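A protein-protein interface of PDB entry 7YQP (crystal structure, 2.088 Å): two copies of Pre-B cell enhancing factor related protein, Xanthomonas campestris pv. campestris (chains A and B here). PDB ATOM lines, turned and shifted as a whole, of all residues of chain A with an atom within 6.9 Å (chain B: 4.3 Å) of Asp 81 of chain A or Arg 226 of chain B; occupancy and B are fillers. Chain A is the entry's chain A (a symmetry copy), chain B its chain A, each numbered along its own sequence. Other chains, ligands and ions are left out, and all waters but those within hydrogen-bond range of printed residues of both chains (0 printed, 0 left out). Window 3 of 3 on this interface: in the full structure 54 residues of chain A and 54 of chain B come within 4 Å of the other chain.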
ATOM      1  N   TYR A  17     -10.015 -13.031 -37.620  1.00  0.00           N
ATOM      2  CA  TYR A  17     -10.306 -12.470 -36.304  1.00  0.00           C
ATOM      3  C   TYR A  17      -9.740 -13.312 -35.166  1.00  0.00           C
ATOM      4  O   TYR A  17      -9.665 -12.827 -34.033  1.00  0.00           O
ATOM      5  CB  TYR A  17     -11.814 -12.296 -36.125  1.00  0.00           C
ATOM      6  CG  TYR A  17     -12.591 -13.587 -35.972  1.00  0.00           C
ATOM      7  CD1 TYR A  17     -12.970 -14.331 -37.082  1.00  0.00           C
ATOM      8  CD2 TYR A  17     -12.962 -14.052 -34.717  1.00  0.00           C
ATOM      9  CE1 TYR A  17     -13.684 -15.508 -36.943  1.00  0.00           C
ATOM     10  CE2 TYR A  17     -13.677 -15.222 -34.570  1.00  0.00           C
ATOM     11  CZ  TYR A  17     -14.033 -15.948 -35.684  1.00  0.00           C
ATOM     12  OH  TYR A  17     -14.742 -17.119 -35.533  1.00  0.00           O
ATOM     13  N   ASP A  19      -6.633 -14.648 -35.506  1.00  0.00           N
ATOM     14  CA  ASP A  19      -5.207 -14.707 -35.832  1.00  0.00           C
ATOM     15  C   ASP A  19      -4.405 -13.865 -34.838  1.00  0.00           C
ATOM     16  O   ASP A  19      -3.866 -12.799 -35.151  1.00  0.00           O
ATOM     17  CB  ASP A  19      -4.981 -14.247 -37.266  1.00  0.00           C
ATOM     18  CG  ASP A  19      -3.527 -14.312 -37.678  1.00  0.00           C
ATOM     19  OD1 ASP A  19      -2.785 -15.143 -37.114  1.00  0.00           O
ATOM     20  OD2 ASP A  19      -3.124 -13.526 -38.561  1.00  0.00           O
ATOM     21  N   ASN A  20      -4.340 -14.366 -33.602  1.00  0.00           N
ATOM     22  CA  ASN A  20      -3.463 -13.779 -32.588  1.00  0.00           C
ATOM     23  C   ASN A  20      -3.197 -14.868 -31.551  1.00  0.00           C
ATOM     24  O   ASN A  20      -4.063 -15.151 -30.717  1.00  0.00           O
ATOM     25  CB  ASN A  20      -4.072 -12.540 -31.953  1.00  0.00           C
ATOM     26  CG  ASN A  20      -3.103 -11.833 -31.013  1.00  0.00           C
ATOM     27  OD1 ASN A  20      -2.064 -12.383 -30.639  1.00  0.00           O
ATOM     28  ND2 ASN A  20      -3.436 -10.607 -30.635  1.00  0.00           N
ATOM     29  N   LEU A  23      -3.820 -14.430 -27.761  1.00  0.00           N
ATOM     30  CA  LEU A  23      -5.187 -14.536 -27.274  1.00  0.00           C
ATOM     31  C   LEU A  23      -5.788 -15.919 -27.502  1.00  0.00           C
ATOM     32  O   LEU A  23      -6.985 -16.110 -27.266  1.00  0.00           O
ATOM     33  CB  LEU A  23      -6.060 -13.469 -27.932  1.00  0.00           C
ATOM     34  CG  LEU A  23      -5.600 -12.029 -27.682  1.00  0.00           C
ATOM     35  CD1 LEU A  23      -6.281 -11.064 -28.644  1.00  0.00           C
ATOM     36  CD2 LEU A  23      -5.860 -11.622 -26.240  1.00  0.00           C
ATOM     37  N   HIS A  76       4.619  -7.163 -32.763  1.00  0.00           N
ATOM     38  CA  HIS A  76       4.252  -6.090 -31.843  1.00  0.00           C
ATOM     39  C   HIS A  76       2.772  -5.753 -31.953  1.00  0.00           C
ATOM     40  O   HIS A  76       2.162  -5.312 -30.972  1.00  0.00           O
ATOM     41  CB  HIS A  76       5.103  -4.849 -32.114  1.00  0.00           C
ATOM     42  CG  HIS A  76       6.516  -4.967 -31.629  1.00  0.00           C
ATOM     43  ND1 HIS A  76       6.836  -5.106 -30.295  1.00  0.00           N
ATOM     44  CD2 HIS A  76       7.693  -4.960 -32.299  1.00  0.00           C
ATOM     45  CE1 HIS A  76       8.149  -5.183 -30.166  1.00  0.00           C
ATOM     46  NE2 HIS A  76       8.693  -5.095 -31.366  1.00  0.00           N
ATOM     47  N   ALA A  77       2.181  -5.956 -33.132  1.00  0.00           N
ATOM     48  CA  ALA A  77       0.744  -5.763 -33.287  1.00  0.00           C
ATOM     49  C   ALA A  77      -0.030  -6.749 -32.423  1.00  0.00           C
ATOM     50  O   ALA A  77      -0.968  -6.366 -31.713  1.00  0.00           O
ATOM     51  CB  ALA A  77       0.353  -5.910 -34.759  1.00  0.00           C
ATOM     52  N   ASP A  78       0.345  -8.032 -32.481  1.00  0.00           N
ATOM     53  CA  ASP A  78      -0.246  -9.026 -31.589  1.00  0.00           C
ATOM     54  C   ASP A  78      -0.170  -8.568 -30.139  1.00  0.00           C
ATOM     55  O   ASP A  78      -1.121  -8.744 -29.368  1.00  0.00           O
ATOM     56  CB  ASP A  78       0.468 -10.373 -31.742  1.00  0.00           C
ATOM     57  CG  ASP A  78       0.292 -10.987 -33.120  1.00  0.00           C
ATOM     58  OD1 ASP A  78      -0.678 -10.632 -33.821  1.00  0.00           O
ATOM     59  OD2 ASP A  78       1.130 -11.837 -33.499  1.00  0.00           O
ATOM     60  N   ILE A  79       0.957  -7.968 -29.757  1.00  0.00           N
ATOM     61  CA  ILE A  79       1.168  -7.581 -28.367  1.00  0.00           C
ATOM     62  C   ILE A  79       0.291  -6.391 -28.005  1.00  0.00           C
ATOM     63  O   ILE A  79      -0.339  -6.369 -26.941  1.00  0.00           O
ATOM     64  CB  ILE A  79       2.658  -7.286 -28.122  1.00  0.00           C
ATOM     65  CG1 ILE A  79       3.479  -8.563 -28.306  1.00  0.00           C
ATOM     66  CG2 ILE A  79       2.865  -6.692 -26.733  1.00  0.00           C
ATOM     67  CD1 ILE A  79       4.960  -8.350 -28.190  1.00  0.00           C
ATOM     68  N   ASP A  80       0.243  -5.381 -28.880  1.00  0.00           N
ATOM     69  CA  ASP A  80      -0.633  -4.236 -28.650  1.00  0.00           C
ATOM     70  C   ASP A  80      -2.077  -4.684 -28.470  1.00  0.00           C
ATOM     71  O   ASP A  80      -2.759  -4.265 -27.528  1.00  0.00           O
ATOM     72  CB  ASP A  80      -0.528  -3.246 -29.811  1.00  0.00           C
ATOM     73  CG  ASP A  80       0.869  -2.696 -29.989  1.00  0.00           C
ATOM     74  OD1 ASP A  80       1.597  -2.572 -28.983  1.00  0.00           O
ATOM     75  OD2 ASP A  80       1.237  -2.387 -31.142  1.00  0.00           O
ATOM     76  N   ASP A  81      -2.553  -5.552 -29.364  1.00  0.00           N
ATOM     77  CA  ASP A  81      -3.936  -6.014 -29.297  1.00  0.00           C
ATOM     78  C   ASP A  81      -4.198  -6.787 -28.010  1.00  0.00           C
ATOM     79  O   ASP A  81      -5.196  -6.542 -27.321  1.00  0.00           O
ATOM     80  CB  ASP A  81      -4.254  -6.875 -30.517  1.00  0.00           C
ATOM     81  CG  ASP A  81      -5.670  -7.412 -30.497  1.00  0.00           C
ATOM     82  OD1 ASP A  81      -6.568  -6.709 -29.988  1.00  0.00           O
ATOM     83  OD2 ASP A  81      -5.884  -8.541 -30.988  1.00  0.00           O
ATOM     84  N   ALA A  82      -3.311  -7.724 -27.668  1.00  0.00           N
ATOM     85  CA  ALA A  82      -3.502  -8.521 -26.458  1.00  0.00           C
ATOM     86  C   ALA A  82      -3.442  -7.652 -25.207  1.00  0.00           C
ATOM     87  O   ALA A  82      -4.304  -7.757 -24.325  1.00  0.00           O
ATOM     88  CB  ALA A  82      -2.456  -9.635 -26.394  1.00  0.00           C
ATOM     89  N   LYS A  83      -2.426  -6.789 -25.109  1.00  0.00           N
ATOM     90  CA  LYS A  83      -2.318  -5.875 -23.974  1.00  0.00           C
ATOM     91  C   LYS A  83      -3.618  -5.113 -23.754  1.00  0.00           C
ATOM     92  O   LYS A  83      -4.108  -5.003 -22.623  1.00  0.00           O
ATOM     93  CB  LYS A  83      -1.159  -4.901 -24.196  1.00  0.00           C
ATOM     94  CG  LYS A  83      -0.997  -3.858 -23.111  1.00  0.00           C
ATOM     95  CD  LYS A  83      -0.088  -2.726 -23.567  1.00  0.00           C
ATOM     96  CE  LYS A  83       0.253  -1.792 -22.418  1.00  0.00           C
ATOM     97  NZ  LYS A  83       0.962  -0.571 -22.892  1.00  0.00           N
ATOM     98  N   ALA A  84      -4.199  -4.587 -24.833  1.00  0.00           N
ATOM     99  CA  ALA A  84      -5.412  -3.787 -24.704  1.00  0.00           C
ATOM    100  C   ALA A  84      -6.598  -4.646 -24.287  1.00  0.00           C
ATOM    101  O   ALA A  84      -7.281  -4.339 -23.305  1.00  0.00           O
ATOM    102  CB  ALA A  84      -5.707  -3.065 -26.017  1.00  0.00           C
ATOM    103  N   LEU A  85      -6.858  -5.731 -25.022  1.00  0.00           N
ATOM    104  CA  LEU A  85      -8.038  -6.547 -24.747  1.00  0.00           C
ATOM    105  C   LEU A  85      -8.012  -7.101 -23.328  1.00  0.00           C
ATOM    106  O   LEU A  85      -9.034  -7.090 -22.631  1.00  0.00           O
ATOM    107  CB  LEU A  85      -8.133  -7.692 -25.757  1.00  0.00           C
ATOM    108  CG  LEU A  85      -9.279  -8.694 -25.575  1.00  0.00           C
ATOM    109  CD1 LEU A  85     -10.606  -7.980 -25.380  1.00  0.00           C
ATOM    110  CD2 LEU A  85      -9.357  -9.639 -26.756  1.00  0.00           C
ATOM    111  N   LEU A  86      -6.854  -7.589 -22.883  1.00  0.00           N
ATOM    112  CA  LEU A  86      -6.794  -8.275 -21.596  1.00  0.00           C
ATOM    113  C   LEU A  86      -6.871  -7.317 -20.414  1.00  0.00           C
ATOM    114  O   LEU A  86      -7.376  -7.698 -19.349  1.00  0.00           O
ATOM    115  CB  LEU A  86      -5.525  -9.127 -21.508  1.00  0.00           C
ATOM    116  CG  LEU A  86      -5.585 -10.369 -22.396  1.00  0.00           C
ATOM    117  CD1 LEU A  86      -4.243 -10.667 -23.079  1.00  0.00           C
ATOM    118  CD2 LEU A  86      -6.096 -11.562 -21.594  1.00  0.00           C
ATOM    119  N   ALA A  87      -6.393  -6.082 -20.573  1.00  0.00           N
ATOM    120  CA  ALA A  87      -6.548  -5.101 -19.506  1.00  0.00           C
ATOM    121  C   ALA A  87      -8.018  -4.794 -19.268  1.00  0.00           C
ATOM    122  O   ALA A  87      -8.480  -4.756 -18.122  1.00  0.00           O
ATOM    123  CB  ALA A  87      -5.778  -3.824 -19.840  1.00  0.00           C
ATOM    124  N   PHE A  93      -0.994  -8.937 -18.131  1.00  0.00           N
ATOM    125  CA  PHE A  93      -0.384  -9.358 -19.382  1.00  0.00           C
ATOM    126  C   PHE A  93       1.092  -8.998 -19.368  1.00  0.00           C
ATOM    127  O   PHE A  93       1.448  -7.845 -19.110  1.00  0.00           O
ATOM    128  CB  PHE A  93      -1.086  -8.708 -20.575  1.00  0.00           C
ATOM    129  CG  PHE A  93      -0.502  -9.086 -21.899  1.00  0.00           C
ATOM    130  CD1 PHE A  93      -0.594 -10.385 -22.364  1.00  0.00           C
ATOM    131  CD2 PHE A  93       0.144  -8.140 -22.680  1.00  0.00           C
ATOM    132  CE1 PHE A  93      -0.055 -10.735 -23.584  1.00  0.00           C
ATOM    133  CE2 PHE A  93       0.684  -8.485 -23.901  1.00  0.00           C
ATOM    134  CZ  PHE A  93       0.584  -9.783 -24.354  1.00  0.00           C
ATOM    135  N   ARG A  99       7.339  -8.702 -25.696  1.00  0.00           N
ATOM    136  CA  ARG A  99       8.157  -7.845 -26.546  1.00  0.00           C
ATOM    137  C   ARG A  99       9.592  -8.343 -26.611  1.00  0.00           C
ATOM    138  O   ARG A  99      10.254  -8.195 -27.645  1.00  0.00           O
ATOM    139  CB  ARG A  99       8.111  -6.404 -26.045  1.00  0.00           C
ATOM    140  CG  ARG A  99       6.740  -5.773 -26.190  1.00  0.00           C
ATOM    141  CD  ARG A  99       6.797  -4.259 -26.197  1.00  0.00           C
ATOM    142  NE  ARG A  99       5.456  -3.687 -26.113  1.00  0.00           N
ATOM    143  CZ  ARG A  99       4.597  -3.631 -27.128  1.00  0.00           C
ATOM    144  NH1 ARG A  99       4.937  -4.105 -28.320  1.00  0.00           N
ATOM    145  NH2 ARG A  99       3.396  -3.097 -26.952  1.00  0.00           N
ATOM    146  N   LEU B 222     -14.263 -13.703 -26.779  1.00  0.00           N
ATOM    147  CA  LEU B 222     -14.215 -12.252 -26.918  1.00  0.00           C
ATOM    148  C   LEU B 222     -13.852 -11.852 -28.340  1.00  0.00           C
ATOM    149  O   LEU B 222     -14.347 -10.844 -28.854  1.00  0.00           O
ATOM    150  CB  LEU B 222     -13.214 -11.662 -25.925  1.00  0.00           C
ATOM    151  CG  LEU B 222     -13.274 -12.229 -24.506  1.00  0.00           C
ATOM    152  CD1 LEU B 222     -12.200 -11.602 -23.625  1.00  0.00           C
ATOM    153  CD2 LEU B 222     -14.659 -12.027 -23.904  1.00  0.00           C
ATOM    154  N   LEU B 223     -12.992 -12.633 -28.995  1.00  0.00           N
ATOM    155  CA  LEU B 223     -12.609 -12.305 -30.362  1.00  0.00           C
ATOM    156  C   LEU B 223     -13.783 -12.471 -31.319  1.00  0.00           C
ATOM    157  O   LEU B 223     -13.986 -11.636 -32.210  1.00  0.00           O
ATOM    158  CB  LEU B 223     -11.427 -13.174 -30.790  1.00  0.00           C
ATOM    159  CG  LEU B 223     -10.143 -12.831 -30.030  1.00  0.00           C
ATOM    160  CD1 LEU B 223      -9.158 -13.989 -30.062  1.00  0.00           C
ATOM    161  CD2 LEU B 223      -9.512 -11.566 -30.589  1.00  0.00           C
ATOM    162  N   LEU B 224     -14.578 -13.533 -31.146  1.00  0.00           N
ATOM    163  CA  LEU B 224     -15.721 -13.747 -32.028  1.00  0.00           C
ATOM    164  C   LEU B 224     -16.803 -12.703 -31.786  1.00  0.00           C
ATOM    165  O   LEU B 224     -17.362 -12.142 -32.735  1.00  0.00           O
ATOM    166  CB  LEU B 224     -16.284 -15.155 -31.838  1.00  0.00           C
ATOM    167  CG  LEU B 224     -17.405 -15.563 -32.801  1.00  0.00           C
ATOM    168  CD1 LEU B 224     -17.222 -17.005 -33.251  1.00  0.00           C
ATOM    169  CD2 LEU B 224     -18.783 -15.365 -32.172  1.00  0.00           C
ATOM    170  N   ALA B 225     -17.112 -12.430 -30.517  1.00  0.00           N
ATOM    171  CA  ALA B 225     -18.158 -11.461 -30.208  1.00  0.00           C
ATOM    172  C   ALA B 225     -17.791 -10.071 -30.710  1.00  0.00           C
ATOM    173  O   ALA B 225     -18.660  -9.319 -31.167  1.00  0.00           O
ATOM    174  CB  ALA B 225     -18.423 -11.437 -28.705  1.00  0.00           C
ATOM    175  N   ARG B 226     -16.509  -9.707 -30.636  1.00  0.00           N
ATOM    176  CA  ARG B 226     -16.098  -8.408 -31.149  1.00  0.00           C
ATOM    177  C   ARG B 226     -15.971  -8.402 -32.664  1.00  0.00           C
ATOM    178  O   ARG B 226     -16.037  -7.330 -33.274  1.00  0.00           O
ATOM    179  CB  ARG B 226     -14.787  -7.963 -30.491  1.00  0.00           C
ATOM    180  CG  ARG B 226     -13.499  -8.459 -31.127  1.00  0.00           C
ATOM    181  CD  ARG B 226     -12.320  -7.665 -30.562  1.00  0.00           C
ATOM    182  NE  ARG B 226     -11.024  -8.151 -31.028  1.00  0.00           N
ATOM    183  CZ  ARG B 226      -9.861  -7.820 -30.473  1.00  0.00           C
ATOM    184  NH1 ARG B 226      -9.830  -7.001 -29.430  1.00  0.00           N
ATOM    185  NH2 ARG B 226      -8.728  -8.308 -30.959  1.00  0.00           N
ATOM    186  N   ALA B 227     -15.817  -9.569 -33.285  1.00  0.00           N
ATOM    187  CA  ALA B 227     -15.757  -9.658 -34.737  1.00  0.00           C
ATOM    188  C   ALA B 227     -17.123  -9.842 -35.378  1.00  0.00           C
ATOM    189  O   ALA B 227     -17.349  -9.337 -36.483  1.00  0.00           O
ATOM    190  CB  ALA B 227     -14.850 -10.814 -35.160  1.00  0.00           C
ATOM    191  N   HIS B 228     -18.042 -10.552 -34.716  1.00  0.00           N
ATOM    192  CA  HIS B 228     -19.327 -10.887 -35.316  1.00  0.00           C
ATOM    193  C   HIS B 228     -20.533 -10.269 -34.628  1.00  0.00           C
ATOM    194  O   HIS B 228     -21.568 -10.106 -35.282  1.00  0.00           O
ATOM    195  CB  HIS B 228     -19.523 -12.412 -35.354  1.00  0.00           C
ATOM    196  CG  HIS B 228     -18.521 -13.126 -36.206  1.00  0.00           C
ATOM    197  ND1 HIS B 228     -18.208 -14.458 -36.032  1.00  0.00           N
ATOM    198  CD2 HIS B 228     -17.757 -12.692 -37.236  1.00  0.00           C
ATOM    199  CE1 HIS B 228     -17.297 -14.813 -36.920  1.00  0.00           C
ATOM    200  NE2 HIS B 228     -17.006 -13.760 -37.662  1.00  0.00           N
ATOM    201  N   THR B 231     -19.234  -6.365 -30.223  1.00  0.00           N
ATOM    202  CA  THR B 231     -19.045  -6.200 -28.782  1.00  0.00           C
ATOM    203  C   THR B 231     -17.558  -6.229 -28.455  1.00  0.00           C
ATOM    204  O   THR B 231     -16.973  -7.318 -28.328  1.00  0.00           O
ATOM    205  CB  THR B 231     -19.801  -7.276 -28.014  1.00  0.00           C
ATOM    206  OG1 THR B 231     -21.180  -7.244 -28.400  1.00  0.00           O
ATOM    207  CG2 THR B 231     -19.700  -7.036 -26.514  1.00  0.00           C
ATOM    208  N   PRO B 232     -16.922  -5.061 -28.299  1.00  0.00           N
ATOM    209  CA  PRO B 232     -15.458  -5.030 -28.101  1.00  0.00           C
ATOM    210  C   PRO B 232     -14.932  -5.967 -27.025  1.00  0.00           C
ATOM    211  O   PRO B 232     -13.935  -6.658 -27.254  1.00  0.00           O
ATOM    212  CB  PRO B 232     -15.199  -3.557 -27.756  1.00  0.00           C
ATOM    213  CG  PRO B 232     -16.278  -2.817 -28.482  1.00  0.00           C
ATOM    214  CD  PRO B 232     -17.498  -3.709 -28.423  1.00  0.00           C
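Of chain A, only Asp 81 and Leu 85 come within 4 Å of Arg 226 of chain B.
Of the printed residues of chain A, Leu 224 of chain B touches Tyr 17 (3.4 Å).
Printed residues of chain A within 4 Å of Leu 223 of chain B: Tyr 17 (3.6 Å) and Leu 23 (3.8 Å).
Printed residues of chain A within 4 Å of His 228 of chain B: Tyr 17.
Of the printed residues of chain B, Tyr 17 of chain A touches Leu 223, Leu 224, Ala 227 and His 228.
Printed residues of chain B within 4 Å of Leu 85 of chain A: Arg 226 (3.8 Å).
The nearest printed residue of chain B that does not touch Asp 81 of chain A is Leu 223 of chain B (4.7 Å).
OD2 of Asp 81 of chain A lies within salt-bridge range of NH2 of Arg 226 of chain B (2.9 Å).
O of Thr 231 of chain B sits close to N of Arg 226 of chain B.
The side-chain amide nitrogen of Asn 20 of chain A sits at hydrogen-bond distance from the side-chain carboxylate of Asp 81 of chain A (3.2 Å).
Of the 9 printed residues of chain B, 5 touch a printed residue of chain A.
Hydrophobic or aromatic side chains of chain A within 4 Å of the printed part of chain B: Tyr 17, Leu 23 and Leu 85.
Among the printed residues, Asp or Glu carboxylates within 4 Å of a Lys or Arg side-chain nitrogen of the other chain: Asp 81 of chain A with Arg 226 of chain B (2.9 Å).
Among the printed residues, merely in contact across the chains: Tyr 17 of chain A with Leu 223 of chain B (3.6 Å), Tyr 17 of chain A with Leu 224 of chain B (3.4 Å), Tyr 17 of chain A with Ala 227 of chain B (3.5 Å), Tyr 17 of chain A with His 228 of chain B (3.7 Å), Leu 23 of chain A with Leu 223 of chain B (3.8 Å) and Leu 85 of chain A with Arg 226 of chain B (3.8 Å).
No position is printed for both chains.
Of the 7 pairs that touch across the chains among the printed residues, none has its exchanged pair printed and touching as well.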
